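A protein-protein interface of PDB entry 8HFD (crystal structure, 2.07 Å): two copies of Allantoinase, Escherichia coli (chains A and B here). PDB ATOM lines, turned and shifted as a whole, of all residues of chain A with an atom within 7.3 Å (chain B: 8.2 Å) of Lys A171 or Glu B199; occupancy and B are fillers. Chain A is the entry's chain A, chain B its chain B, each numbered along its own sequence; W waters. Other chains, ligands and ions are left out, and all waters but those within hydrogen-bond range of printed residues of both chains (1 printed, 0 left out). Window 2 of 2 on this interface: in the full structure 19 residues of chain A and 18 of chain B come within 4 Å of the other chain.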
ATOM      1  N   LEU A 126      13.455   7.411 -14.355  1.00  0.00           N
ATOM      2  CA  LEU A 126      13.179   6.653 -15.573  1.00  0.00           C
ATOM      3  C   LEU A 126      14.106   7.238 -16.631  1.00  0.00           C
ATOM      4  O   LEU A 126      13.901   8.357 -17.111  1.00  0.00           O
ATOM      5  CB  LEU A 126      11.712   6.754 -15.973  1.00  0.00           C
ATOM      6  CG  LEU A 126      11.414   6.483 -17.453  1.00  0.00           C
ATOM      7  CD1 LEU A 126      11.794   5.037 -17.852  1.00  0.00           C
ATOM      8  CD2 LEU A 126       9.939   6.744 -17.717  1.00  0.00           C
ATOM      9  N   ILE A 131      15.243   0.915 -18.197  1.00  0.00           N
ATOM     10  CA  ILE A 131      13.842   0.591 -18.453  1.00  0.00           C
ATOM     11  C   ILE A 131      13.540  -0.856 -18.110  1.00  0.00           C
ATOM     12  O   ILE A 131      12.413  -1.186 -17.735  1.00  0.00           O
ATOM     13  CB  ILE A 131      13.472   0.903 -19.909  1.00  0.00           C
ATOM     14  CG1 ILE A 131      13.735   2.380 -20.199  1.00  0.00           C
ATOM     15  CG2 ILE A 131      12.026   0.527 -20.156  1.00  0.00           C
ATOM     16  CD1 ILE A 131      12.922   2.929 -21.320  1.00  0.00           C
ATOM     17  N   ASP A 132      14.523  -1.741 -18.230  1.00  0.00           N
ATOM     18  CA  ASP A 132      14.307  -3.146 -17.922  1.00  0.00           C
ATOM     19  C   ASP A 132      14.449  -3.452 -16.440  1.00  0.00           C
ATOM     20  O   ASP A 132      14.212  -4.598 -16.039  1.00  0.00           O
ATOM     21  CB  ASP A 132      15.277  -4.007 -18.731  1.00  0.00           C
ATOM     22  CG  ASP A 132      15.149  -3.776 -20.228  1.00  0.00           C
ATOM     23  OD1 ASP A 132      14.006  -3.796 -20.737  1.00  0.00           O
ATOM     24  OD2 ASP A 132      16.197  -3.579 -20.898  1.00  0.00           O
ATOM     25  N   LEU A 134      13.129  -1.233 -13.818  1.00  0.00           N
ATOM     26  CA  LEU A 134      12.314  -0.314 -13.028  1.00  0.00           C
ATOM     27  C   LEU A 134      11.725  -0.996 -11.799  1.00  0.00           C
ATOM     28  O   LEU A 134      11.395  -0.317 -10.821  1.00  0.00           O
ATOM     29  CB  LEU A 134      11.194   0.292 -13.891  1.00  0.00           C
ATOM     30  CG  LEU A 134      11.610   1.150 -15.100  1.00  0.00           C
ATOM     31  CD1 LEU A 134      10.418   1.607 -15.925  1.00  0.00           C
ATOM     32  CD2 LEU A 134      12.429   2.367 -14.668  1.00  0.00           C
ATOM     33  N   ASN A 165      13.752   8.948 -24.860  1.00  0.00           N
ATOM     34  CA  ASN A 165      13.090   9.256 -26.148  1.00  0.00           C
ATOM     35  C   ASN A 165      11.626   8.809 -26.028  1.00  0.00           C
ATOM     36  O   ASN A 165      11.282   8.231 -24.995  1.00  0.00           O
ATOM     37  CB  ASN A 165      13.842   8.646 -27.332  1.00  0.00           C
ATOM     38  CG  ASN A 165      13.944   7.137 -27.309  1.00  0.00           C
ATOM     39  OD1 ASN A 165      12.992   6.444 -26.971  1.00  0.00           O
ATOM     40  ND2 ASN A 165      15.092   6.617 -27.706  1.00  0.00           N
ATOM     41  N   ASP A 166      10.812   9.051 -27.053  1.00  0.00           N
ATOM     42  CA  ASP A 166       9.364   8.713 -27.008  1.00  0.00           C
ATOM     43  C   ASP A 166       9.172   7.220 -26.720  1.00  0.00           C
ATOM     44  O   ASP A 166       8.280   6.879 -25.947  1.00  0.00           O
ATOM     45  CB  ASP A 166       8.660   9.126 -28.303  1.00  0.00           C
ATOM     46  CG  ASP A 166       8.675  10.621 -28.589  1.00  0.00           C
ATOM     47  OD1 ASP A 166       8.918  11.404 -27.652  1.00  0.00           O
ATOM     48  OD2 ASP A 166       8.441  10.990 -29.749  1.00  0.00           O
ATOM     49  N   TRP A 167       9.988   6.387 -27.347  1.00  0.00           N
ATOM     50  CA  TRP A 167       9.872   4.923 -27.164  1.00  0.00           C
ATOM     51  C   TRP A 167      10.151   4.580 -25.704  1.00  0.00           C
ATOM     52  O   TRP A 167       9.336   3.893 -25.102  1.00  0.00           O
ATOM     53  CB  TRP A 167      10.837   4.190 -28.097  1.00  0.00           C
ATOM     54  CG  TRP A 167      10.989   2.747 -27.744  1.00  0.00           C
ATOM     55  CD1 TRP A 167      12.123   2.105 -27.344  1.00  0.00           C
ATOM     56  CD2 TRP A 167       9.943   1.765 -27.733  1.00  0.00           C
ATOM     57  NE1 TRP A 167      11.856   0.787 -27.099  1.00  0.00           N
ATOM     58  CE2 TRP A 167      10.527   0.549 -27.327  1.00  0.00           C
ATOM     59  CE3 TRP A 167       8.578   1.794 -28.032  1.00  0.00           C
ATOM     60  CZ2 TRP A 167       9.790  -0.625 -27.220  1.00  0.00           C
ATOM     61  CZ3 TRP A 167       7.849   0.634 -27.915  1.00  0.00           C
ATOM     62  CH2 TRP A 167       8.450  -0.557 -27.518  1.00  0.00           C
ATOM     63  N   GLN A 168      11.267   5.080 -25.186  1.00  0.00           N
ATOM     64  CA  GLN A 168      11.694   4.778 -23.800  1.00  0.00           C
ATOM     65  C   GLN A 168      10.622   5.271 -22.816  1.00  0.00           C
ATOM     66  O   GLN A 168      10.287   4.521 -21.904  1.00  0.00           O
ATOM     67  CB  GLN A 168      13.095   5.355 -23.602  1.00  0.00           C
ATOM     68  CG  GLN A 168      14.173   4.620 -24.382  1.00  0.00           C
ATOM     69  CD  GLN A 168      15.420   5.439 -24.605  1.00  0.00           C
ATOM     70  OE1 GLN A 168      15.452   6.643 -24.376  1.00  0.00           O
ATOM     71  NE2 GLN A 168      16.468   4.782 -25.065  1.00  0.00           N
ATOM     72  N   PHE A 169      10.085   6.464 -23.042  1.00  0.00           N
ATOM     73  CA  PHE A 169       8.988   6.971 -22.188  1.00  0.00           C
ATOM     74  C   PHE A 169       7.813   5.988 -22.245  1.00  0.00           C
ATOM     75  O   PHE A 169       7.371   5.546 -21.203  1.00  0.00           O
ATOM     76  CB  PHE A 169       8.547   8.376 -22.600  1.00  0.00           C
ATOM     77  CG  PHE A 169       7.377   8.882 -21.799  1.00  0.00           C
ATOM     78  CD1 PHE A 169       7.552   9.309 -20.495  1.00  0.00           C
ATOM     79  CD2 PHE A 169       6.099   8.882 -22.329  1.00  0.00           C
ATOM     80  CE1 PHE A 169       6.477   9.757 -19.747  1.00  0.00           C
ATOM     81  CE2 PHE A 169       5.025   9.330 -21.578  1.00  0.00           C
ATOM     82  CZ  PHE A 169       5.217   9.765 -20.290  1.00  0.00           C
ATOM     83  N   PHE A 170       7.335   5.679 -23.449  1.00  0.00           N
ATOM     84  CA  PHE A 170       6.165   4.782 -23.604  1.00  0.00           C
ATOM     85  C   PHE A 170       6.399   3.422 -22.934  1.00  0.00           C
ATOM     86  O   PHE A 170       5.514   2.984 -22.203  1.00  0.00           O
ATOM     87  CB  PHE A 170       5.788   4.591 -25.073  1.00  0.00           C
ATOM     88  CG  PHE A 170       4.670   3.600 -25.264  1.00  0.00           C
ATOM     89  CD1 PHE A 170       3.365   3.939 -24.949  1.00  0.00           C
ATOM     90  CD2 PHE A 170       4.928   2.318 -25.716  1.00  0.00           C
ATOM     91  CE1 PHE A 170       2.336   3.027 -25.110  1.00  0.00           C
ATOM     92  CE2 PHE A 170       3.899   1.407 -25.874  1.00  0.00           C
ATOM     93  CZ  PHE A 170       2.607   1.762 -25.569  1.00  0.00           C
ATOM     94  N   LYS A 171       7.531   2.781 -23.209  1.00  0.00           N
ATOM     95  CA  LYS A 171       7.800   1.430 -22.650  1.00  0.00           C
ATOM     96  C   LYS A 171       7.918   1.518 -21.124  1.00  0.00           C
ATOM     97  O   LYS A 171       7.327   0.681 -20.447  1.00  0.00           O
ATOM     98  CB  LYS A 171       9.048   0.790 -23.259  1.00  0.00           C
ATOM     99  CG  LYS A 171       9.080  -0.729 -23.228  1.00  0.00           C
ATOM    100  CD  LYS A 171       8.043  -1.367 -24.126  1.00  0.00           C
ATOM    101  CE  LYS A 171       8.370  -2.803 -24.468  1.00  0.00           C
ATOM    102  NZ  LYS A 171       7.188  -3.530 -24.980  1.00  0.00           N
ATOM    103  N   GLY A 172       8.663   2.501 -20.626  1.00  0.00           N
ATOM    104  CA  GLY A 172       8.795   2.691 -19.170  1.00  0.00           C
ATOM    105  C   GLY A 172       7.464   2.995 -18.527  1.00  0.00           C
ATOM    106  O   GLY A 172       7.159   2.391 -17.510  1.00  0.00           O
ATOM    107  N   ALA A 173       6.717   3.916 -19.127  1.00  0.00           N
ATOM    108  CA  ALA A 173       5.382   4.281 -18.609  1.00  0.00           C
ATOM    109  C   ALA A 173       4.502   3.031 -18.522  1.00  0.00           C
ATOM    110  O   ALA A 173       3.837   2.870 -17.511  1.00  0.00           O
ATOM    111  CB  ALA A 173       4.742   5.327 -19.471  1.00  0.00           C
ATOM    112  N   GLN A 174       4.534   2.193 -19.553  1.00  0.00           N
ATOM    113  CA  GLN A 174       3.751   0.935 -19.565  1.00  0.00           C
ATOM    114  C   GLN A 174       4.115   0.092 -18.341  1.00  0.00           C
ATOM    115  O   GLN A 174       3.217  -0.362 -17.652  1.00  0.00           O
ATOM    116  CB  GLN A 174       4.041   0.178 -20.858  1.00  0.00           C
ATOM    117  CG  GLN A 174       2.849  -0.584 -21.414  1.00  0.00           C
ATOM    118  CD  GLN A 174       3.030  -0.953 -22.866  1.00  0.00           C
ATOM    119  OE1 GLN A 174       2.066  -1.188 -23.588  1.00  0.00           O
ATOM    120  NE2 GLN A 174       4.275  -1.010 -23.308  1.00  0.00           N
ATOM    121  N   LYS A 175       5.410  -0.066 -18.098  1.00  0.00           N
ATOM    122  CA  LYS A 175       5.887  -0.889 -16.966  1.00  0.00           C
ATOM    123  C   LYS A 175       5.501  -0.219 -15.649  1.00  0.00           C
ATOM    124  O   LYS A 175       5.069  -0.936 -14.751  1.00  0.00           O
ATOM    125  CB  LYS A 175       7.391  -1.101 -17.088  1.00  0.00           C
ATOM    126  CG  LYS A 175       7.955  -2.178 -16.176  1.00  0.00           C
ATOM    127  CD  LYS A 175       7.091  -3.418 -16.138  1.00  0.00           C
ATOM    128  CE  LYS A 175       6.948  -3.995 -14.747  1.00  0.00           C
ATOM    129  NZ  LYS A 175       8.128  -4.807 -14.369  1.00  0.00           N
ATOM    130  N   LEU A 176       5.629   1.109 -15.573  1.00  0.00           N
ATOM    131  CA  LEU A 176       5.244   1.866 -14.355  1.00  0.00           C
ATOM    132  C   LEU A 176       3.745   1.697 -14.095  1.00  0.00           C
ATOM    133  O   LEU A 176       3.384   1.440 -12.948  1.00  0.00           O
ATOM    134  CB  LEU A 176       5.646   3.334 -14.526  1.00  0.00           C
ATOM    135  CG  LEU A 176       7.150   3.598 -14.581  1.00  0.00           C
ATOM    136  CD1 LEU A 176       7.443   5.087 -14.590  1.00  0.00           C
ATOM    137  CD2 LEU A 176       7.866   2.922 -13.427  1.00  0.00           C
ATOM    138  N   GLY A 177       2.921   1.790 -15.134  1.00  0.00           N
ATOM    139  CA  GLY A 177       1.473   1.552 -14.987  1.00  0.00           C
ATOM    140  C   GLY A 177       1.204   0.188 -14.384  1.00  0.00           C
ATOM    141  O   GLY A 177       0.371   0.103 -13.493  1.00  0.00           O
ATOM    142  N   ALA A 234      -0.095   4.280 -22.617  1.00  0.00           N
ATOM    143  CA  ALA A 234       0.636   3.316 -21.804  1.00  0.00           C
ATOM    144  C   ALA A 234      -0.101   2.947 -20.525  1.00  0.00           C
ATOM    145  O   ALA A 234       0.287   1.977 -19.868  1.00  0.00           O
ATOM    146  CB  ALA A 234       2.025   3.846 -21.444  1.00  0.00           C
ATOM    147  N   ILE B 192       8.908   5.071 -32.315  1.00  0.00           N
ATOM    148  CA  ILE B 192       8.140   3.998 -31.690  1.00  0.00           C
ATOM    149  C   ILE B 192       7.875   2.873 -32.685  1.00  0.00           C
ATOM    150  O   ILE B 192       7.963   1.687 -32.337  1.00  0.00           O
ATOM    151  CB  ILE B 192       6.844   4.569 -31.093  1.00  0.00           C
ATOM    152  CG1 ILE B 192       7.197   5.609 -30.016  1.00  0.00           C
ATOM    153  CG2 ILE B 192       5.966   3.446 -30.541  1.00  0.00           C
ATOM    154  CD1 ILE B 192       5.978   6.204 -29.301  1.00  0.00           C
ATOM    155  N   CYS B 193       7.569   3.221 -33.947  1.00  0.00           N
ATOM    156  CA  CYS B 193       7.363   2.196 -34.972  1.00  0.00           C
ATOM    157  C   CYS B 193       8.641   1.392 -35.233  1.00  0.00           C
ATOM    158  O   CYS B 193       8.590   0.168 -35.398  1.00  0.00           O
ATOM    159  CB  CYS B 193       6.865   2.847 -36.265  1.00  0.00           C
ATOM    160  SG  CYS B 193       5.170   3.489 -36.110  1.00  0.00           S
ATOM    161  N   ASP B 194       9.791   2.062 -35.293  1.00  0.00           N
ATOM    162  CA  ASP B 194      11.049   1.348 -35.506  1.00  0.00           C
ATOM    163  C   ASP B 194      11.361   0.419 -34.331  1.00  0.00           C
ATOM    164  O   ASP B 194      11.656  -0.765 -34.526  1.00  0.00           O
ATOM    165  CB  ASP B 194      12.188   2.347 -35.727  1.00  0.00           C
ATOM    166  CG  ASP B 194      12.083   3.082 -37.054  1.00  0.00           C
ATOM    167  OD1 ASP B 194      11.316   2.643 -37.946  1.00  0.00           O
ATOM    168  OD2 ASP B 194      12.769   4.112 -37.201  1.00  0.00           O
ATOM    169  N   GLU B 195      11.278   0.930 -33.097  1.00  0.00           N
ATOM    170  CA  GLU B 195      11.612   0.111 -31.933  1.00  0.00           C
ATOM    171  C   GLU B 195      10.630  -1.042 -31.757  1.00  0.00           C
ATOM    172  O   GLU B 195      11.036  -2.160 -31.408  1.00  0.00           O
ATOM    173  CB  GLU B 195      11.661   0.970 -30.668  1.00  0.00           C
ATOM    174  CG  GLU B 195      12.804   1.946 -30.659  1.00  0.00           C
ATOM    175  CD  GLU B 195      14.167   1.269 -30.522  1.00  0.00           C
ATOM    176  OE1 GLU B 195      14.229   0.020 -30.408  1.00  0.00           O
ATOM    177  OE2 GLU B 195      15.181   1.999 -30.529  1.00  0.00           O
ATOM    178  N   LEU B 196       9.334  -0.801 -31.984  1.00  0.00           N
ATOM    179  CA  LEU B 196       8.393  -1.921 -31.945  1.00  0.00           C
ATOM    180  C   LEU B 196       8.718  -2.943 -33.035  1.00  0.00           C
ATOM    181  O   LEU B 196       8.546  -4.148 -32.834  1.00  0.00           O
ATOM    182  CB  LEU B 196       6.949  -1.424 -32.085  1.00  0.00           C
ATOM    183  CG  LEU B 196       6.320  -0.782 -30.841  1.00  0.00           C
ATOM    184  CD1 LEU B 196       4.929  -0.239 -31.143  1.00  0.00           C
ATOM    185  CD2 LEU B 196       6.267  -1.815 -29.712  1.00  0.00           C
ATOM    186  N   GLY B 197       9.204  -2.476 -34.191  1.00  0.00           N
ATOM    187  CA  GLY B 197       9.569  -3.406 -35.251  1.00  0.00           C
ATOM    188  C   GLY B 197      10.750  -4.287 -34.876  1.00  0.00           C
ATOM    189  O   GLY B 197      10.707  -5.503 -35.044  1.00  0.00           O
ATOM    190  N   GLU B 198      11.832  -3.679 -34.383  1.00  0.00           N
ATOM    191  CA  GLU B 198      12.972  -4.464 -33.909  1.00  0.00           C
ATOM    192  C   GLU B 198      12.537  -5.479 -32.866  1.00  0.00           C
ATOM    193  O   GLU B 198      12.952  -6.641 -32.896  1.00  0.00           O
ATOM    194  CB  GLU B 198      14.042  -3.533 -33.338  1.00  0.00           C
ATOM    195  CG  GLU B 198      14.603  -2.576 -34.379  1.00  0.00           C
ATOM    196  CD  GLU B 198      15.072  -3.307 -35.623  1.00  0.00           C
ATOM    197  OE1 GLU B 198      15.919  -4.218 -35.469  1.00  0.00           O
ATOM    198  OE2 GLU B 198      14.601  -2.980 -36.745  1.00  0.00           O
ATOM    199  N   GLU B 199      11.687  -5.052 -31.939  1.00  0.00           N
ATOM    200  CA  GLU B 199      11.153  -5.955 -30.929  1.00  0.00           C
ATOM    201  C   GLU B 199      10.472  -7.163 -31.564  1.00  0.00           C
ATOM    202  O   GLU B 199      10.712  -8.308 -31.164  1.00  0.00           O
ATOM    203  CB  GLU B 199      10.181  -5.179 -30.046  1.00  0.00           C
ATOM    204  CG  GLU B 199       9.829  -5.824 -28.744  1.00  0.00           C
ATOM    205  CD  GLU B 199       9.086  -4.857 -27.840  1.00  0.00           C
ATOM    206  OE1 GLU B 199       7.835  -4.811 -27.899  1.00  0.00           O
ATOM    207  OE2 GLU B 199       9.771  -4.130 -27.094  1.00  0.00           O
ATOM    208  N   ALA B 200       9.598  -6.925 -32.546  1.00  0.00           N
ATOM    209  CA  ALA B 200       8.933  -8.033 -33.224  1.00  0.00           C
ATOM    210  C   ALA B 200       9.946  -8.926 -33.917  1.00  0.00           C
ATOM    211  O   ALA B 200       9.852 -10.158 -33.844  1.00  0.00           O
ATOM    212  CB  ALA B 200       7.918  -7.509 -34.232  1.00  0.00           C
ATOM    213  N   LYS B 201      10.928  -8.321 -34.587  1.00  0.00           N
ATOM    214  CA  LYS B 201      11.972  -9.094 -35.245  1.00  0.00           C
ATOM    215  C   LYS B 201      12.680 -10.000 -34.250  1.00  0.00           C
ATOM    216  O   LYS B 201      12.790 -11.211 -34.465  1.00  0.00           O
ATOM    217  CB  LYS B 201      12.973  -8.155 -35.922  1.00  0.00           C
ATOM    218  CG  LYS B 201      12.653  -7.828 -37.359  1.00  0.00           C
ATOM    219  CD  LYS B 201      12.764  -6.339 -37.619  1.00  0.00           C
ATOM    220  CE  LYS B 201      14.081  -5.984 -38.263  1.00  0.00           C
ATOM    221  NZ  LYS B 201      13.995  -4.676 -38.969  1.00  0.00           N
ATOM    222  N   ARG B 202      13.153  -9.427 -33.138  1.00  0.00           N
ATOM    223  CA  ARG B 202      13.883 -10.208 -32.148  1.00  0.00           C
ATOM    224  C   ARG B 202      13.054 -11.369 -31.623  1.00  0.00           C
ATOM    225  O   ARG B 202      13.607 -12.407 -31.241  1.00  0.00           O
ATOM    226  CB  ARG B 202      14.322  -9.305 -30.996  1.00  0.00           C
ATOM    227  CG  ARG B 202      15.383  -8.311 -31.381  1.00  0.00           C
ATOM    228  CD  ARG B 202      15.958  -7.618 -30.144  1.00  0.00           C
ATOM    229  NE  ARG B 202      14.994  -6.714 -29.525  1.00  0.00           N
ATOM    230  CZ  ARG B 202      14.980  -5.399 -29.700  1.00  0.00           C
ATOM    231  NH1 ARG B 202      15.888  -4.790 -30.446  1.00  0.00           N
ATOM    232  NH2 ARG B 202      14.038  -4.673 -29.106  1.00  0.00           N
ATOM    233  N   GLU B 203      11.739 -11.216 -31.574  1.00  0.00           N
ATOM    234  CA  GLU B 203      10.889 -12.295 -31.100  1.00  0.00           C
ATOM    235  C   GLU B 203      10.545 -13.288 -32.195  1.00  0.00           C
ATOM    236  O   GLU B 203       9.816 -14.246 -31.922  1.00  0.00           O
ATOM    237  CB  GLU B 203       9.593 -11.732 -30.502  1.00  0.00           C
ATOM    238  CG  GLU B 203       9.793 -10.640 -29.447  1.00  0.00           C
ATOM    239  CD  GLU B 203       8.488 -10.243 -28.746  1.00  0.00           C
ATOM    240  OE1 GLU B 203       7.416 -10.769 -29.115  1.00  0.00           O
ATOM    241  OE2 GLU B 203       8.535  -9.406 -27.816  1.00  0.00           O
ATOM    242  N   GLY B 204      11.046 -13.078 -33.414  1.00  0.00           N
ATOM    243  CA  GLY B 204      10.629 -13.877 -34.547  1.00  0.00           C
ATOM    244  C   GLY B 204       9.177 -13.706 -34.921  1.00  0.00           C
ATOM    245  O   GLY B 204       8.585 -14.609 -35.505  1.00  0.00           O
ATOM    246  N   ARG B 205       8.576 -12.573 -34.595  1.00  0.00           N
ATOM    247  CA  ARG B 205       7.174 -12.323 -34.912  1.00  0.00           C
ATOM    248  C   ARG B 205       7.158 -11.454 -36.166  1.00  0.00           C
ATOM    249  O   ARG B 205       7.382 -10.243 -36.093  1.00  0.00           O
ATOM    250  CB  ARG B 205       6.467 -11.656 -33.735  1.00  0.00           C
ATOM    251  CG  ARG B 205       5.941 -12.605 -32.656  1.00  0.00           C
ATOM    252  CD  ARG B 205       5.073 -11.840 -31.658  1.00  0.00           C
ATOM    253  NE  ARG B 205       5.812 -10.736 -31.050  1.00  0.00           N
ATOM    254  CZ  ARG B 205       5.651  -9.450 -31.349  1.00  0.00           C
ATOM    255  NH1 ARG B 205       4.751  -9.049 -32.235  1.00  0.00           N
ATOM    256  NH2 ARG B 205       6.418  -8.543 -30.751  1.00  0.00           N
ATOM    257  N   VAL B 206       6.896 -12.069 -37.325  1.00  0.00           N
ATOM    258  CA  VAL B 206       7.103 -11.371 -38.594  1.00  0.00           C
ATOM    259  C   VAL B 206       5.935 -11.528 -39.560  1.00  0.00           C
ATOM    260  O   VAL B 206       6.110 -11.351 -40.768  1.00  0.00           O
ATOM    261  CB  VAL B 206       8.405 -11.845 -39.275  1.00  0.00           C
ATOM    262  CG1 VAL B 206       9.609 -11.574 -38.387  1.00  0.00           C
ATOM    263  CG2 VAL B 206       8.309 -13.330 -39.638  1.00  0.00           C
ATOM    264  N   ALA B 213       0.735  -4.634 -35.753  1.00  0.00           N
ATOM    265  CA  ALA B 213       0.828  -4.418 -34.314  1.00  0.00           C
ATOM    266  C   ALA B 213       2.035  -3.563 -33.963  1.00  0.00           C
ATOM    267  O   ALA B 213       2.017  -2.870 -32.940  1.00  0.00           O
ATOM    268  CB  ALA B 213       0.886  -5.754 -33.562  1.00  0.00           C
ATOM    269  N   SER B 214       3.078  -3.571 -34.803  1.00  0.00           N
ATOM    270  CA  SER B 214       4.260  -2.758 -34.552  1.00  0.00           C
ATOM    271  C   SER B 214       4.123  -1.330 -35.065  1.00  0.00           C
ATOM    272  O   SER B 214       5.072  -0.550 -34.936  1.00  0.00           O
ATOM    273  CB  SER B 214       5.503  -3.408 -35.172  1.00  0.00           C
ATOM    274  OG  SER B 214       5.633  -3.110 -36.560  1.00  0.00           O
ATOM    275  N   PHE B 218      -1.937   4.483 -32.133  1.00  0.00           N
ATOM    276  CA  PHE B 218      -1.475   5.635 -31.356  1.00  0.00           C
ATOM    277  C   PHE B 218      -0.219   6.262 -31.944  1.00  0.00           C
ATOM    278  O   PHE B 218       0.013   7.450 -31.710  1.00  0.00           O
ATOM    279  CB  PHE B 218      -1.285   5.280 -29.848  1.00  0.00           C
ATOM    280  CG  PHE B 218       0.023   4.615 -29.498  1.00  0.00           C
ATOM    281  CD1 PHE B 218       1.165   5.369 -29.257  1.00  0.00           C
ATOM    282  CD2 PHE B 218       0.095   3.235 -29.361  1.00  0.00           C
ATOM    283  CE1 PHE B 218       2.369   4.750 -28.923  1.00  0.00           C
ATOM    284  CE2 PHE B 218       1.293   2.600 -29.025  1.00  0.00           C
ATOM    285  CZ  PHE B 218       2.434   3.351 -28.810  1.00  0.00           C
ATOM    286  N   MET B 329       8.511  -7.955 -42.147  1.00  0.00           N
ATOM    287  CA  MET B 329       9.138  -6.891 -41.331  1.00  0.00           C
ATOM    288  C   MET B 329      10.340  -6.268 -42.051  1.00  0.00           C
ATOM    289  O   MET B 329      10.525  -5.065 -41.909  1.00  0.00           O
ATOM    290  CB  MET B 329       9.582  -7.442 -39.975  1.00  0.00           C
ATOM    291  CG  MET B 329       8.446  -7.971 -39.124  1.00  0.00           C
ATOM    292  SD  MET B 329       7.290  -6.685 -38.598  1.00  0.00           S
ATOM    293  CE  MET B 329       8.423  -5.368 -38.170  1.00  0.00           C
HETATM  294  O   HOH W   1      15.378   3.780 -28.553  1.00  0.00           O
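NZ of Lys A171 lies within salt-bridge range of OE1 of Glu B199 (3.3 Å).
The side-chain amide oxygen of Asn A165 is in hydrogen-bond range of the backbone NH of Trp A167, at 3.0 Å.
Among the printed residues, merely in contact across the chains: Trp A167 with Ile B192 (3.9 Å), Trp A167 with Glu B195 (3.4 Å), Trp A167 with Leu B196 (3.3 Å), Trp A167 with Glu B199 (3.5 Å) and Phe A170 with Phe B218 (3.6 Å).
Lys A171 touches one residue of chain B.
Of chain A, only Trp A167 and Lys A171 come within 4 Å of Glu B199.
No residue of chain B comes within 4 Å of Gly A172.
Printed residues of chain B within 4 Å of Trp A167: Ile B192, Glu B195, Leu B196 and Glu B199.
Printed residues of chain A within 4 Å of Phe B218: Phe A170 (3.6 Å).
Gly B197 touches none of the printed residues of chain A.
Lys B201 touches none of the printed residues of chain A.
Hydrophobic or aromatic side chains of chain A that line the printed part of chain B: Trp A167 and Phe A170.
Along chain A the printed residues that touch a printed residue of chain B span positions 167 to 171.
Of the 19 printed residues of chain B, 5 touch a printed residue of chain A.
Along chain B the printed residues that touch a printed residue of chain A span positions 192 to 218.
Among the printed residues, 6 pairs touch across the chains.
No position is printed for both chains.
Of the 6 pairs that touch across the chains among the printed residues, none has its exchanged pair printed and touching as well.
Water W1 lies within hydrogen-bond range of OE2 of Glu B195 (2.7 Å) and ND2 of Asn A165 (3.0 Å).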
